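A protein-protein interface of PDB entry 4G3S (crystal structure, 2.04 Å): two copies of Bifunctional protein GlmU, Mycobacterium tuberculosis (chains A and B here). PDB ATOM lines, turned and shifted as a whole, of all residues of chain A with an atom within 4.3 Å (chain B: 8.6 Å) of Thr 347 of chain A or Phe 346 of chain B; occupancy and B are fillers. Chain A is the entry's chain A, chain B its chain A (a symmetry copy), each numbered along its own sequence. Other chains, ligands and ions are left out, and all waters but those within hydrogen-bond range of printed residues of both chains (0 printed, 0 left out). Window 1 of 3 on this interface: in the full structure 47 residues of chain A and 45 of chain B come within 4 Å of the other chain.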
ATOM      1  N   ARG A 329      -6.893 -22.087   5.265  1.00  0.00           N
ATOM      2  CA  ARG A 329      -5.533 -22.465   4.783  1.00  0.00           C
ATOM      3  C   ARG A 329      -4.612 -22.857   5.902  1.00  0.00           C
ATOM      4  O   ARG A 329      -3.542 -22.270   6.106  1.00  0.00           O
ATOM      5  CB  ARG A 329      -4.868 -21.323   4.007  1.00  0.00           C
ATOM      6  CG  ARG A 329      -5.531 -21.080   2.686  1.00  0.00           C
ATOM      7  CD  ARG A 329      -4.753 -20.044   1.947  1.00  0.00           C
ATOM      8  NE  ARG A 329      -5.515 -19.756   0.753  1.00  0.00           N
ATOM      9  CZ  ARG A 329      -5.300 -20.352  -0.397  1.00  0.00           C
ATOM     10  NH1 ARG A 329      -4.357 -21.307  -0.491  1.00  0.00           N
ATOM     11  NH2 ARG A 329      -6.078 -20.050  -1.413  1.00  0.00           N
ATOM     12  N   THR A 330      -5.052 -23.854   6.651  1.00  0.00           N
ATOM     13  CA  THR A 330      -4.369 -24.264   7.846  1.00  0.00           C
ATOM     14  C   THR A 330      -3.991 -25.748   7.657  1.00  0.00           C
ATOM     15  O   THR A 330      -4.756 -26.504   7.131  1.00  0.00           O
ATOM     16  CB  THR A 330      -5.263 -24.040   9.115  1.00  0.00           C
ATOM     17  OG1 THR A 330      -5.410 -22.619   9.348  1.00  0.00           O
ATOM     18  CG2 THR A 330      -4.579 -24.561  10.331  1.00  0.00           C
ATOM     19  N   HIS A 331      -2.791 -26.114   8.103  1.00  0.00           N
ATOM     20  CA  HIS A 331      -2.359 -27.487   8.121  1.00  0.00           C
ATOM     21  C   HIS A 331      -2.177 -27.819   9.609  1.00  0.00           C
ATOM     22  O   HIS A 331      -1.297 -27.236  10.259  1.00  0.00           O
ATOM     23  CB  HIS A 331      -0.979 -27.609   7.421  1.00  0.00           C
ATOM     24  CG  HIS A 331      -0.673 -29.004   6.985  1.00  0.00           C
ATOM     25  ND1 HIS A 331      -1.211 -29.555   5.825  1.00  0.00           N
ATOM     26  CD2 HIS A 331       0.136 -29.954   7.531  1.00  0.00           C
ATOM     27  CE1 HIS A 331      -0.795 -30.813   5.729  1.00  0.00           C
ATOM     28  NE2 HIS A 331       0.034 -31.068   6.737  1.00  0.00           N
ATOM     29  N   VAL A 343      -7.862 -18.781  12.778  1.00  0.00           N
ATOM     30  CA  VAL A 343      -6.552 -19.423  12.447  1.00  0.00           C
ATOM     31  C   VAL A 343      -6.369 -19.296  10.921  1.00  0.00           C
ATOM     32  O   VAL A 343      -7.348 -19.574  10.182  1.00  0.00           O
ATOM     33  CB  VAL A 343      -6.608 -20.940  12.851  1.00  0.00           C
ATOM     34  CG1 VAL A 343      -5.286 -21.692  12.476  1.00  0.00           C
ATOM     35  CG2 VAL A 343      -6.872 -20.973  14.389  1.00  0.00           C
ATOM     36  N   GLY A 344      -5.188 -18.911  10.445  1.00  0.00           N
ATOM     37  CA  GLY A 344      -4.921 -18.906   8.991  1.00  0.00           C
ATOM     38  C   GLY A 344      -5.033 -17.451   8.510  1.00  0.00           C
ATOM     39  O   GLY A 344      -5.271 -16.550   9.327  1.00  0.00           O
ATOM     40  N   PRO A 345      -4.779 -17.188   7.209  1.00  0.00           N
ATOM     41  CA  PRO A 345      -4.348 -18.157   6.262  1.00  0.00           C
ATOM     42  C   PRO A 345      -2.869 -18.473   6.454  1.00  0.00           C
ATOM     43  O   PRO A 345      -2.122 -17.642   6.968  1.00  0.00           O
ATOM     44  CB  PRO A 345      -4.585 -17.509   4.907  1.00  0.00           C
ATOM     45  CG  PRO A 345      -4.387 -16.022   5.190  1.00  0.00           C
ATOM     46  CD  PRO A 345      -4.848 -15.824   6.656  1.00  0.00           C
ATOM     47  N   PHE A 346      -2.482 -19.687   6.090  1.00  0.00           N
ATOM     48  CA  PHE A 346      -1.054 -20.101   6.102  1.00  0.00           C
ATOM     49  C   PHE A 346      -0.514 -20.296   7.525  1.00  0.00           C
ATOM     50  O   PHE A 346       0.418 -19.617   7.936  1.00  0.00           O
ATOM     51  CB  PHE A 346      -0.120 -19.189   5.315  1.00  0.00           C
ATOM     52  CG  PHE A 346      -0.584 -18.866   3.918  1.00  0.00           C
ATOM     53  CD1 PHE A 346      -0.521 -19.806   2.878  1.00  0.00           C
ATOM     54  CD2 PHE A 346      -1.039 -17.602   3.636  1.00  0.00           C
ATOM     55  CE1 PHE A 346      -0.982 -19.435   1.503  1.00  0.00           C
ATOM     56  CE2 PHE A 346      -1.501 -17.263   2.297  1.00  0.00           C
ATOM     57  CZ  PHE A 346      -1.413 -18.165   1.265  1.00  0.00           C
ATOM     58  N   THR A 347      -1.077 -21.294   8.207  1.00  0.00           N
ATOM     59  CA  THR A 347      -0.872 -21.509   9.640  1.00  0.00           C
ATOM     60  C   THR A 347      -0.646 -22.995   9.801  1.00  0.00           C
ATOM     61  O   THR A 347      -1.378 -23.796   9.269  1.00  0.00           O
ATOM     62  CB  THR A 347      -2.087 -21.023  10.517  1.00  0.00           C
ATOM     63  OG1 THR A 347      -2.322 -19.627  10.240  1.00  0.00           O
ATOM     64  CG2 THR A 347      -1.701 -21.184  12.082  1.00  0.00           C
ATOM     65  N   TYR A 348       0.377 -23.325  10.565  1.00  0.00           N
ATOM     66  CA  TYR A 348       0.768 -24.709  10.806  1.00  0.00           C
ATOM     67  C   TYR A 348       0.612 -25.015  12.315  1.00  0.00           C
ATOM     68  O   TYR A 348       1.288 -24.333  13.150  1.00  0.00           O
ATOM     69  CB  TYR A 348       2.237 -24.898  10.403  1.00  0.00           C
ATOM     70  CG  TYR A 348       2.821 -26.328  10.507  1.00  0.00           C
ATOM     71  CD1 TYR A 348       2.016 -27.466  10.467  1.00  0.00           C
ATOM     72  CD2 TYR A 348       4.210 -26.498  10.613  1.00  0.00           C
ATOM     73  CE1 TYR A 348       2.598 -28.768  10.542  1.00  0.00           C
ATOM     74  CE2 TYR A 348       4.784 -27.762  10.716  1.00  0.00           C
ATOM     75  CZ  TYR A 348       3.975 -28.866  10.649  1.00  0.00           C
ATOM     76  OH  TYR A 348       4.603 -30.051  10.776  1.00  0.00           O
ATOM     77  N   LEU A 349      -0.259 -25.995  12.644  1.00  0.00           N
ATOM     78  CA  LEU A 349      -0.426 -26.451  14.065  1.00  0.00           C
ATOM     79  C   LEU A 349       0.126 -27.844  14.219  1.00  0.00           C
ATOM     80  O   LEU A 349      -0.275 -28.748  13.544  1.00  0.00           O
ATOM     81  CB  LEU A 349      -1.920 -26.427  14.538  1.00  0.00           C
ATOM     82  CG  LEU A 349      -2.705 -25.137  14.217  1.00  0.00           C
ATOM     83  CD1 LEU A 349      -4.242 -25.098  14.645  1.00  0.00           C
ATOM     84  CD2 LEU A 349      -1.991 -23.885  14.733  1.00  0.00           C
ATOM     85  N   LEU A 361      -4.419 -17.156  15.634  1.00  0.00           N
ATOM     86  CA  LEU A 361      -3.082 -17.508  15.066  1.00  0.00           C
ATOM     87  C   LEU A 361      -3.054 -17.142  13.588  1.00  0.00           C
ATOM     88  O   LEU A 361      -3.827 -17.696  12.836  1.00  0.00           O
ATOM     89  CB  LEU A 361      -2.824 -19.033  15.271  1.00  0.00           C
ATOM     90  CG  LEU A 361      -2.777 -19.520  16.729  1.00  0.00           C
ATOM     91  CD1 LEU A 361      -2.646 -21.113  16.863  1.00  0.00           C
ATOM     92  CD2 LEU A 361      -1.609 -18.888  17.566  1.00  0.00           C
ATOM     93  N   GLY A 362      -2.224 -16.181  13.178  1.00  0.00           N
ATOM     94  CA  GLY A 362      -2.265 -15.589  11.855  1.00  0.00           C
ATOM     95  C   GLY A 362      -1.356 -16.243  10.822  1.00  0.00           C
ATOM     96  O   GLY A 362      -0.880 -17.395  10.980  1.00  0.00           O
ATOM     97  N   VAL A 365       2.461 -18.450  10.914  1.00  0.00           N
ATOM     98  CA  VAL A 365       2.643 -18.778  12.324  1.00  0.00           C
ATOM     99  C   VAL A 365       2.607 -20.278  12.444  1.00  0.00           C
ATOM    100  O   VAL A 365       1.813 -20.956  11.778  1.00  0.00           O
ATOM    101  CB  VAL A 365       1.503 -18.104  13.165  1.00  0.00           C
ATOM    102  CG1 VAL A 365       1.526 -18.563  14.659  1.00  0.00           C
ATOM    103  CG2 VAL A 365       1.681 -16.565  13.027  1.00  0.00           C
ATOM    104  N   PRO B 312      -0.624 -32.695   0.754  1.00  0.00           N
ATOM    105  CA  PRO B 312      -1.512 -32.100  -0.271  1.00  0.00           C
ATOM    106  C   PRO B 312      -0.970 -30.765  -0.804  1.00  0.00           C
ATOM    107  O   PRO B 312       0.000 -30.231  -0.269  1.00  0.00           O
ATOM    108  CB  PRO B 312      -2.833 -31.881   0.498  1.00  0.00           C
ATOM    109  CG  PRO B 312      -2.349 -31.649   1.990  1.00  0.00           C
ATOM    110  CD  PRO B 312      -1.324 -32.839   2.068  1.00  0.00           C
ATOM    111  N   ASP B 313      -1.571 -30.226  -1.851  1.00  0.00           N
ATOM    112  CA  ASP B 313      -1.282 -28.857  -2.287  1.00  0.00           C
ATOM    113  C   ASP B 313       0.165 -28.578  -2.566  1.00  0.00           C
ATOM    114  O   ASP B 313       0.699 -27.606  -2.067  1.00  0.00           O
ATOM    115  CB  ASP B 313      -1.734 -27.911  -1.202  1.00  0.00           C
ATOM    116  CG  ASP B 313      -3.266 -27.972  -1.006  1.00  0.00           C
ATOM    117  OD1 ASP B 313      -3.989 -28.397  -1.941  1.00  0.00           O
ATOM    118  OD2 ASP B 313      -3.705 -27.575   0.070  1.00  0.00           O
ATOM    119  N   THR B 314       0.825 -29.523  -3.212  1.00  0.00           N
ATOM    120  CA  THR B 314       2.203 -29.370  -3.592  1.00  0.00           C
ATOM    121  C   THR B 314       2.300 -29.176  -5.139  1.00  0.00           C
ATOM    122  O   THR B 314       1.635 -29.894  -5.892  1.00  0.00           O
ATOM    123  CB  THR B 314       2.925 -30.606  -3.119  1.00  0.00           C
ATOM    124  OG1 THR B 314       3.184 -30.465  -1.713  1.00  0.00           O
ATOM    125  CG2 THR B 314       4.299 -30.734  -3.795  1.00  0.00           C
ATOM    126  N   VAL B 327       7.199 -34.326   1.032  1.00  0.00           N
ATOM    127  CA  VAL B 327       7.193 -32.996   0.383  1.00  0.00           C
ATOM    128  C   VAL B 327       5.734 -32.520   0.393  1.00  0.00           C
ATOM    129  O   VAL B 327       4.894 -32.909  -0.474  1.00  0.00           O
ATOM    130  CB  VAL B 327       7.616 -33.136  -1.092  1.00  0.00           C
ATOM    131  CG1 VAL B 327       7.881 -31.770  -1.654  1.00  0.00           C
ATOM    132  CG2 VAL B 327       8.976 -33.950  -1.168  1.00  0.00           C
ATOM    133  N   VAL B 328       5.414 -31.730   1.393  1.00  0.00           N
ATOM    134  CA  VAL B 328       4.035 -31.538   1.766  1.00  0.00           C
ATOM    135  C   VAL B 328       3.811 -29.997   1.573  1.00  0.00           C
ATOM    136  O   VAL B 328       4.660 -29.205   1.969  1.00  0.00           O
ATOM    137  CB  VAL B 328       3.805 -31.952   3.279  1.00  0.00           C
ATOM    138  CG1 VAL B 328       2.419 -31.421   3.701  1.00  0.00           C
ATOM    139  CG2 VAL B 328       3.778 -33.467   3.397  1.00  0.00           C
ATOM    140  N   ARG B 329       2.701 -29.586   0.965  1.00  0.00           N
ATOM    141  CA  ARG B 329       2.399 -28.146   0.717  1.00  0.00           C
ATOM    142  C   ARG B 329       3.617 -27.363   0.320  1.00  0.00           C
ATOM    143  O   ARG B 329       4.004 -26.382   0.968  1.00  0.00           O
ATOM    144  CB  ARG B 329       1.791 -27.472   1.951  1.00  0.00           C
ATOM    145  CG  ARG B 329       0.403 -27.962   2.233  1.00  0.00           C
ATOM    146  CD  ARG B 329      -0.159 -27.173   3.366  1.00  0.00           C
ATOM    147  NE  ARG B 329      -1.433 -27.781   3.676  1.00  0.00           N
ATOM    148  CZ  ARG B 329      -2.571 -27.361   3.173  1.00  0.00           C
ATOM    149  NH1 ARG B 329      -2.580 -26.341   2.295  1.00  0.00           N
ATOM    150  NH2 ARG B 329      -3.671 -28.012   3.484  1.00  0.00           N
ATOM    151  N   THR B 330       4.240 -27.822  -0.752  1.00  0.00           N
ATOM    152  CA  THR B 330       5.497 -27.282  -1.189  1.00  0.00           C
ATOM    153  C   THR B 330       5.284 -26.765  -2.626  1.00  0.00           C
ATOM    154  O   THR B 330       4.614 -27.387  -3.399  1.00  0.00           O
ATOM    155  CB  THR B 330       6.634 -28.360  -1.111  1.00  0.00           C
ATOM    156  OG1 THR B 330       6.920 -28.651   0.278  1.00  0.00           O
ATOM    157  CG2 THR B 330       7.906 -27.812  -1.660  1.00  0.00           C
ATOM    158  N   HIS B 331       5.879 -25.613  -2.935  1.00  0.00           N
ATOM    159  CA  HIS B 331       5.885 -25.081  -4.271  1.00  0.00           C
ATOM    160  C   HIS B 331       7.363 -25.082  -4.685  1.00  0.00           C
ATOM    161  O   HIS B 331       8.164 -24.351  -4.085  1.00  0.00           O
ATOM    162  CB  HIS B 331       5.385 -23.612  -4.249  1.00  0.00           C
ATOM    163  CG  HIS B 331       4.924 -23.138  -5.589  1.00  0.00           C
ATOM    164  ND1 HIS B 331       3.670 -23.463  -6.100  1.00  0.00           N
ATOM    165  CD2 HIS B 331       5.528 -22.340  -6.512  1.00  0.00           C
ATOM    166  CE1 HIS B 331       3.567 -22.938  -7.317  1.00  0.00           C
ATOM    167  NE2 HIS B 331       4.669 -22.242  -7.577  1.00  0.00           N
ATOM    168  N   VAL B 343      10.163 -31.854   3.702  1.00  0.00           N
ATOM    169  CA  VAL B 343       9.990 -30.463   3.178  1.00  0.00           C
ATOM    170  C   VAL B 343       8.515 -30.080   3.416  1.00  0.00           C
ATOM    171  O   VAL B 343       7.630 -30.921   3.117  1.00  0.00           O
ATOM    172  CB  VAL B 343      10.299 -30.455   1.638  1.00  0.00           C
ATOM    173  CG1 VAL B 343      10.078 -29.038   1.007  1.00  0.00           C
ATOM    174  CG2 VAL B 343      11.779 -30.927   1.486  1.00  0.00           C
ATOM    175  N   GLY B 344       8.236 -28.879   3.914  1.00  0.00           N
ATOM    176  CA  GLY B 344       6.838 -28.412   4.032  1.00  0.00           C
ATOM    177  C   GLY B 344       6.425 -28.572   5.503  1.00  0.00           C
ATOM    178  O   GLY B 344       7.246 -28.992   6.330  1.00  0.00           O
ATOM    179  N   PRO B 345       5.190 -28.160   5.867  1.00  0.00           N
ATOM    180  CA  PRO B 345       4.264 -27.525   4.994  1.00  0.00           C
ATOM    181  C   PRO B 345       4.650 -26.067   4.773  1.00  0.00           C
ATOM    182  O   PRO B 345       5.311 -25.468   5.619  1.00  0.00           O
ATOM    183  CB  PRO B 345       2.926 -27.622   5.710  1.00  0.00           C
ATOM    184  CG  PRO B 345       3.315 -27.584   7.187  1.00  0.00           C
ATOM    185  CD  PRO B 345       4.708 -28.259   7.255  1.00  0.00           C
ATOM    186  N   PHE B 346       4.281 -25.539   3.615  1.00  0.00           N
ATOM    187  CA  PHE B 346       4.477 -24.098   3.303  1.00  0.00           C
ATOM    188  C   PHE B 346       5.949 -23.748   3.056  1.00  0.00           C
ATOM    189  O   PHE B 346       6.526 -22.939   3.771  1.00  0.00           O
ATOM    190  CB  PHE B 346       3.882 -23.138   4.329  1.00  0.00           C
ATOM    191  CG  PHE B 346       2.453 -23.427   4.707  1.00  0.00           C
ATOM    192  CD1 PHE B 346       1.383 -23.144   3.843  1.00  0.00           C
ATOM    193  CD2 PHE B 346       2.177 -23.937   5.952  1.00  0.00           C
ATOM    194  CE1 PHE B 346      -0.022 -23.438   4.269  1.00  0.00           C
ATOM    195  CE2 PHE B 346       0.805 -24.232   6.343  1.00  0.00           C
ATOM    196  CZ  PHE B 346      -0.251 -23.930   5.518  1.00  0.00           C
ATOM    197  N   THR B 347       6.488 -24.320   1.978  1.00  0.00           N
ATOM    198  CA  THR B 347       7.923 -24.300   1.686  1.00  0.00           C
ATOM    199  C   THR B 347       8.035 -23.981   0.212  1.00  0.00           C
ATOM    200  O   THR B 347       7.359 -24.566  -0.603  1.00  0.00           O
ATOM    201  CB  THR B 347       8.640 -25.661   2.027  1.00  0.00           C
ATOM    202  OG1 THR B 347       8.407 -25.965   3.418  1.00  0.00           O
ATOM    203  CG2 THR B 347      10.233 -25.485   1.793  1.00  0.00           C
ATOM    204  N   TYR B 348       8.918 -23.052  -0.093  1.00  0.00           N
ATOM    205  CA  TYR B 348       9.138 -22.590  -1.459  1.00  0.00           C
ATOM    206  C   TYR B 348      10.591 -22.930  -1.872  1.00  0.00           C
ATOM    207  O   TYR B 348      11.549 -22.434  -1.199  1.00  0.00           O
ATOM    208  CB  TYR B 348       8.941 -21.069  -1.516  1.00  0.00           C
ATOM    209  CG  TYR B 348       9.051 -20.393  -2.905  1.00  0.00           C
ATOM    210  CD1 TYR B 348       8.834 -21.092  -4.093  1.00  0.00           C
ATOM    211  CD2 TYR B 348       9.347 -19.024  -2.982  1.00  0.00           C
ATOM    212  CE1 TYR B 348       8.922 -20.424  -5.351  1.00  0.00           C
ATOM    213  CE2 TYR B 348       9.464 -18.371  -4.206  1.00  0.00           C
ATOM    214  CZ  TYR B 348       9.221 -19.072  -5.359  1.00  0.00           C
ATOM    215  OH  TYR B 348       9.373 -18.376  -6.502  1.00  0.00           O
ATOM    216  N   LEU B 349      10.736 -23.758  -2.931  1.00  0.00           N
ATOM    217  CA  LEU B 349      12.092 -24.085  -3.488  1.00  0.00           C
ATOM    218  C   LEU B 349      12.249 -23.451  -4.846  1.00  0.00           C
ATOM    219  O   LEU B 349      11.476 -23.681  -5.730  1.00  0.00           O
ATOM    220  CB  LEU B 349      12.346 -25.628  -3.601  1.00  0.00           C
ATOM    221  CG  LEU B 349      11.985 -26.460  -2.352  1.00  0.00           C
ATOM    222  CD1 LEU B 349      12.189 -28.040  -2.450  1.00  0.00           C
ATOM    223  CD2 LEU B 349      12.665 -25.927  -1.089  1.00  0.00           C
ATOM    224  N   LEU B 361      13.568 -28.983   5.379  1.00  0.00           N
ATOM    225  CA  LEU B 361      13.181 -27.556   5.160  1.00  0.00           C
ATOM    226  C   LEU B 361      11.745 -27.351   5.622  1.00  0.00           C
ATOM    227  O   LEU B 361      10.860 -27.965   5.065  1.00  0.00           O
ATOM    228  CB  LEU B 361      13.338 -27.209   3.648  1.00  0.00           C
ATOM    229  CG  LEU B 361      14.759 -27.329   3.072  1.00  0.00           C
ATOM    230  CD1 LEU B 361      14.825 -27.091   1.487  1.00  0.00           C
ATOM    231  CD2 LEU B 361      15.788 -26.342   3.730  1.00  0.00           C
ATOM    232  N   GLY B 362      11.511 -26.551   6.664  1.00  0.00           N
ATOM    233  CA  GLY B 362      10.229 -26.454   7.337  1.00  0.00           C
ATOM    234  C   GLY B 362       9.305 -25.360   6.817  1.00  0.00           C
ATOM    235  O   GLY B 362       9.467 -24.822   5.694  1.00  0.00           O
ATOM    236  N   ALA B 363       8.352 -25.033   7.665  1.00  0.00           N
ATOM    237  CA  ALA B 363       7.329 -24.103   7.334  1.00  0.00           C
ATOM    238  C   ALA B 363       7.813 -22.718   7.249  1.00  0.00           C
ATOM    239  O   ALA B 363       8.564 -22.230   8.106  1.00  0.00           O
ATOM    240  CB  ALA B 363       6.157 -24.223   8.373  1.00  0.00           C
ATOM    241  N   PHE B 364       7.371 -22.044   6.206  1.00  0.00           N
ATOM    242  CA  PHE B 364       7.735 -20.675   5.924  1.00  0.00           C
ATOM    243  C   PHE B 364       9.254 -20.499   5.666  1.00  0.00           C
ATOM    244  O   PHE B 364       9.844 -19.516   6.089  1.00  0.00           O
ATOM    245  CB  PHE B 364       7.120 -19.716   7.003  1.00  0.00           C
ATOM    246  CG  PHE B 364       5.778 -20.202   7.508  1.00  0.00           C
ATOM    247  CD1 PHE B 364       4.715 -20.390   6.597  1.00  0.00           C
ATOM    248  CD2 PHE B 364       5.605 -20.523   8.866  1.00  0.00           C
ATOM    249  CE1 PHE B 364       3.500 -20.896   7.013  1.00  0.00           C
ATOM    250  CE2 PHE B 364       4.406 -20.987   9.337  1.00  0.00           C
ATOM    251  CZ  PHE B 364       3.348 -21.197   8.415  1.00  0.00           C
ATOM    252  N   VAL B 365       9.827 -21.431   4.885  1.00  0.00           N
ATOM    253  CA  VAL B 365      11.228 -21.422   4.479  1.00  0.00           C
ATOM    254  C   VAL B 365      11.261 -21.355   2.976  1.00  0.00           C
ATOM    255  O   VAL B 365      10.452 -21.992   2.289  1.00  0.00           O
ATOM    256  CB  VAL B 365      11.931 -22.719   5.016  1.00  0.00           C
ATOM    257  CG1 VAL B 365      13.387 -22.868   4.463  1.00  0.00           C
ATOM    258  CG2 VAL B 365      11.904 -22.646   6.568  1.00  0.00           C
ATOM    259  N   GLU B 366      12.094 -20.464   2.467  1.00  0.00           N
ATOM    260  CA  GLU B 366      12.278 -20.385   1.046  1.00  0.00           C
ATOM    261  C   GLU B 366      13.791 -20.638   0.875  1.00  0.00           C
ATOM    262  O   GLU B 366      14.635 -20.066   1.661  1.00  0.00           O
ATOM    263  CB  GLU B 366      11.959 -18.944   0.591  1.00  0.00           C
ATOM    264  CG  GLU B 366      12.401 -18.683  -0.866  1.00  0.00           C
ATOM    265  CD  GLU B 366      12.031 -17.306  -1.422  1.00  0.00           C
ATOM    266  OE1 GLU B 366      11.030 -16.692  -0.924  1.00  0.00           O
ATOM    267  OE2 GLU B 366      12.722 -16.844  -2.392  1.00  0.00           O
ATOM    268  N   PRO B 379      14.341 -25.310   9.878  1.00  0.00           N
ATOM    269  CA  PRO B 379      12.925 -25.615  10.107  1.00  0.00           C
ATOM    270  C   PRO B 379      11.916 -24.455  10.096  1.00  0.00           C
ATOM    271  O   PRO B 379      10.721 -24.727   9.973  1.00  0.00           O
ATOM    272  CB  PRO B 379      12.942 -26.219  11.493  1.00  0.00           C
ATOM    273  CG  PRO B 379      14.140 -25.584  12.198  1.00  0.00           C
ATOM    274  CD  PRO B 379      15.169 -25.452  11.098  1.00  0.00           C
ATOM    275  N   HIS B 380      12.327 -23.193  10.263  1.00  0.00           N
ATOM    276  CA  HIS B 380      11.278 -22.152  10.435  1.00  0.00           C
ATOM    277  C   HIS B 380      11.613 -20.788   9.908  1.00  0.00           C
ATOM    278  O   HIS B 380      12.696 -20.253  10.209  1.00  0.00           O
ATOM    279  CB  HIS B 380      10.992 -21.883  11.927  1.00  0.00           C
ATOM    280  CG  HIS B 380      10.817 -23.112  12.769  1.00  0.00           C
ATOM    281  ND1 HIS B 380       9.649 -23.842  12.797  1.00  0.00           N
ATOM    282  CD2 HIS B 380      11.620 -23.663  13.705  1.00  0.00           C
ATOM    283  CE1 HIS B 380       9.774 -24.844  13.651  1.00  0.00           C
ATOM    284  NE2 HIS B 380      10.961 -24.759  14.217  1.00  0.00           N
ATOM    285  N   LEU B 381      10.674 -20.219   9.147  1.00  0.00           N
ATOM    286  CA  LEU B 381      10.618 -18.775   8.838  1.00  0.00           C
ATOM    287  C   LEU B 381      11.984 -18.249   8.385  1.00  0.00           C
ATOM    288  O   LEU B 381      12.470 -17.228   8.892  1.00  0.00           O
ATOM    289  CB  LEU B 381      10.194 -18.004  10.100  1.00  0.00           C
ATOM    290  CG  LEU B 381       8.728 -18.319  10.490  1.00  0.00           C
ATOM    291  CD1 LEU B 381       8.434 -18.247  12.014  1.00  0.00           C
ATOM    292  CD2 LEU B 381       7.782 -17.383   9.706  1.00  0.00           C
ATOM    293  N   THR B 382      12.605 -18.932   7.447  1.00  0.00           N
ATOM    294  CA  THR B 382      13.927 -18.506   7.044  1.00  0.00           C
ATOM    295  C   THR B 382      14.109 -18.442   5.529  1.00  0.00           C
ATOM    296  O   THR B 382      13.534 -19.224   4.781  1.00  0.00           O
ATOM    297  CB  THR B 382      15.080 -19.326   7.783  1.00  0.00           C
ATOM    298  OG1 THR B 382      15.003 -19.588   9.186  1.00  0.00           O
ATOM    299  CG2 THR B 382      16.296 -19.643   7.070  1.00  0.00           C
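The side-chain carboxylate (OD2) of Asp 313 of chain B lies within salt-bridge range of the guanidinium group (NH1) of Arg 329 of chain B.
O of Ala 363 of chain B sits at hydrogen-bond distance from N of Leu 381 of chain B, at 3.1 Å.
The backbone NH (N) of His 331 of chain A sits at hydrogen-bond distance from the backbone carbonyl oxygen (O) of Thr 347 of chain A, 3.0 Å away.
The backbone carbonyl oxygen of Val 328 of chain B is in hydrogen-bond range of the side-chain hydroxyl of Thr 330 of chain B, at 2.9 Å.
O of Arg 329 of chain B sits at hydrogen-bond distance from N of Thr 347 of chain B (3.4 Å).
O of Phe 364 of chain B lies within hydrogen-bond range of N of Thr 382 of chain B, 3.1 Å away.
Arg 329 of chain A touches Phe 346 of chain B.
His 331 of chain A touches Val 328 of chain B (CE1 to CG1, 3.8 Å).
CD2 of His 331 of chain A touches CG of Pro 345 of chain B, 3.98 Å away.
Phe 346 of chain B touches His 331 of chain A.
Phe 346 of chain A touches Phe 346 of chain B.
Phe 364 of chain B touches Phe 346 of chain A.
O of Thr 347 of chain A touches CE2 of Phe 346 of chain B (3.7 Å).
Pro 345 of chain B touches Tyr 348 of chain A.
CD2 of Tyr 348 of chain A touches CB of Ala 363 of chain B, 3.7 Å away.
Val 365 of chain A touches Phe 364 of chain B.
Thr 347 of chain A touches one residue of chain B.
Phe 346 of chain B touches just these residues of chain A: Arg 329 (3.7 Å), His 331 (3.97 Å), Phe 346 (3.9 Å) and Thr 347 (3.7 Å).
No residue of chain B comes within 4 Å of Gly 362 of chain A.
Printed residues of chain B within 4 Å of Tyr 348 of chain A: Pro 345 (3.5 Å) and Ala 363 (3.7 Å).
Of the printed residues of chain B, Arg 329 of chain A touches Phe 346.
Printed residues of chain B within 4 Å of Val 365 of chain A: Phe 364 (3.6 Å).
Printed residues of chain A within 4 Å of Arg 329 of chain B: His 331.
Val 343 of chain B touches none of the printed residues of chain A.
The guanidinium group of Arg 329 of chain B lies within hydrogen-bond range of a ring nitrogen (ND1) of His 331 of chain A, 2.8 Å away.
His 331 of chain A touches Arg 329 of chain B, but with the chains exchanged Arg 329 of chain A does not touch His 331 of chain B (10.0 Å).
His 331 of chain A touches Pro 345 of chain B, but with the chains exchanged Pro 345 of chain A does not touch His 331 of chain B (14.5 Å).
Phe 346 of chain B touches its own counterpart, Phe 346 of chain A.
Tyr 348 of chain A touches Pro 345 of chain B, but with the chains exchanged Pro 345 of chain A does not touch Tyr 348 of chain B (14.2 Å).
Positions printed for both chains: 329, 330, 331, 343, 344, 345, 346, 347, 348, 349, 361, 362 and 365.
Of the 11 pairs that touch across the chains among the printed residues, 1 has its exchanged pair printed and touching as well.
Of the 25 printed residues of chain B, 6 touch a printed residue of chain A.
Hydrophobic or aromatic side chains of chain B that line the printed part of chain A: Val 328, Pro 345, Phe 346, Ala 363 and Phe 364.
Hydrophobic or aromatic side chains of chain A within 4 Å of the printed part of chain B: His 331, Phe 346 and Tyr 348.
Among the printed residues, 11 pairs touch across the chains.
Among the printed residues, no Asp or Glu carboxylate lies within 4 Å of a Lys or Arg side-chain nitrogen of the other chain.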
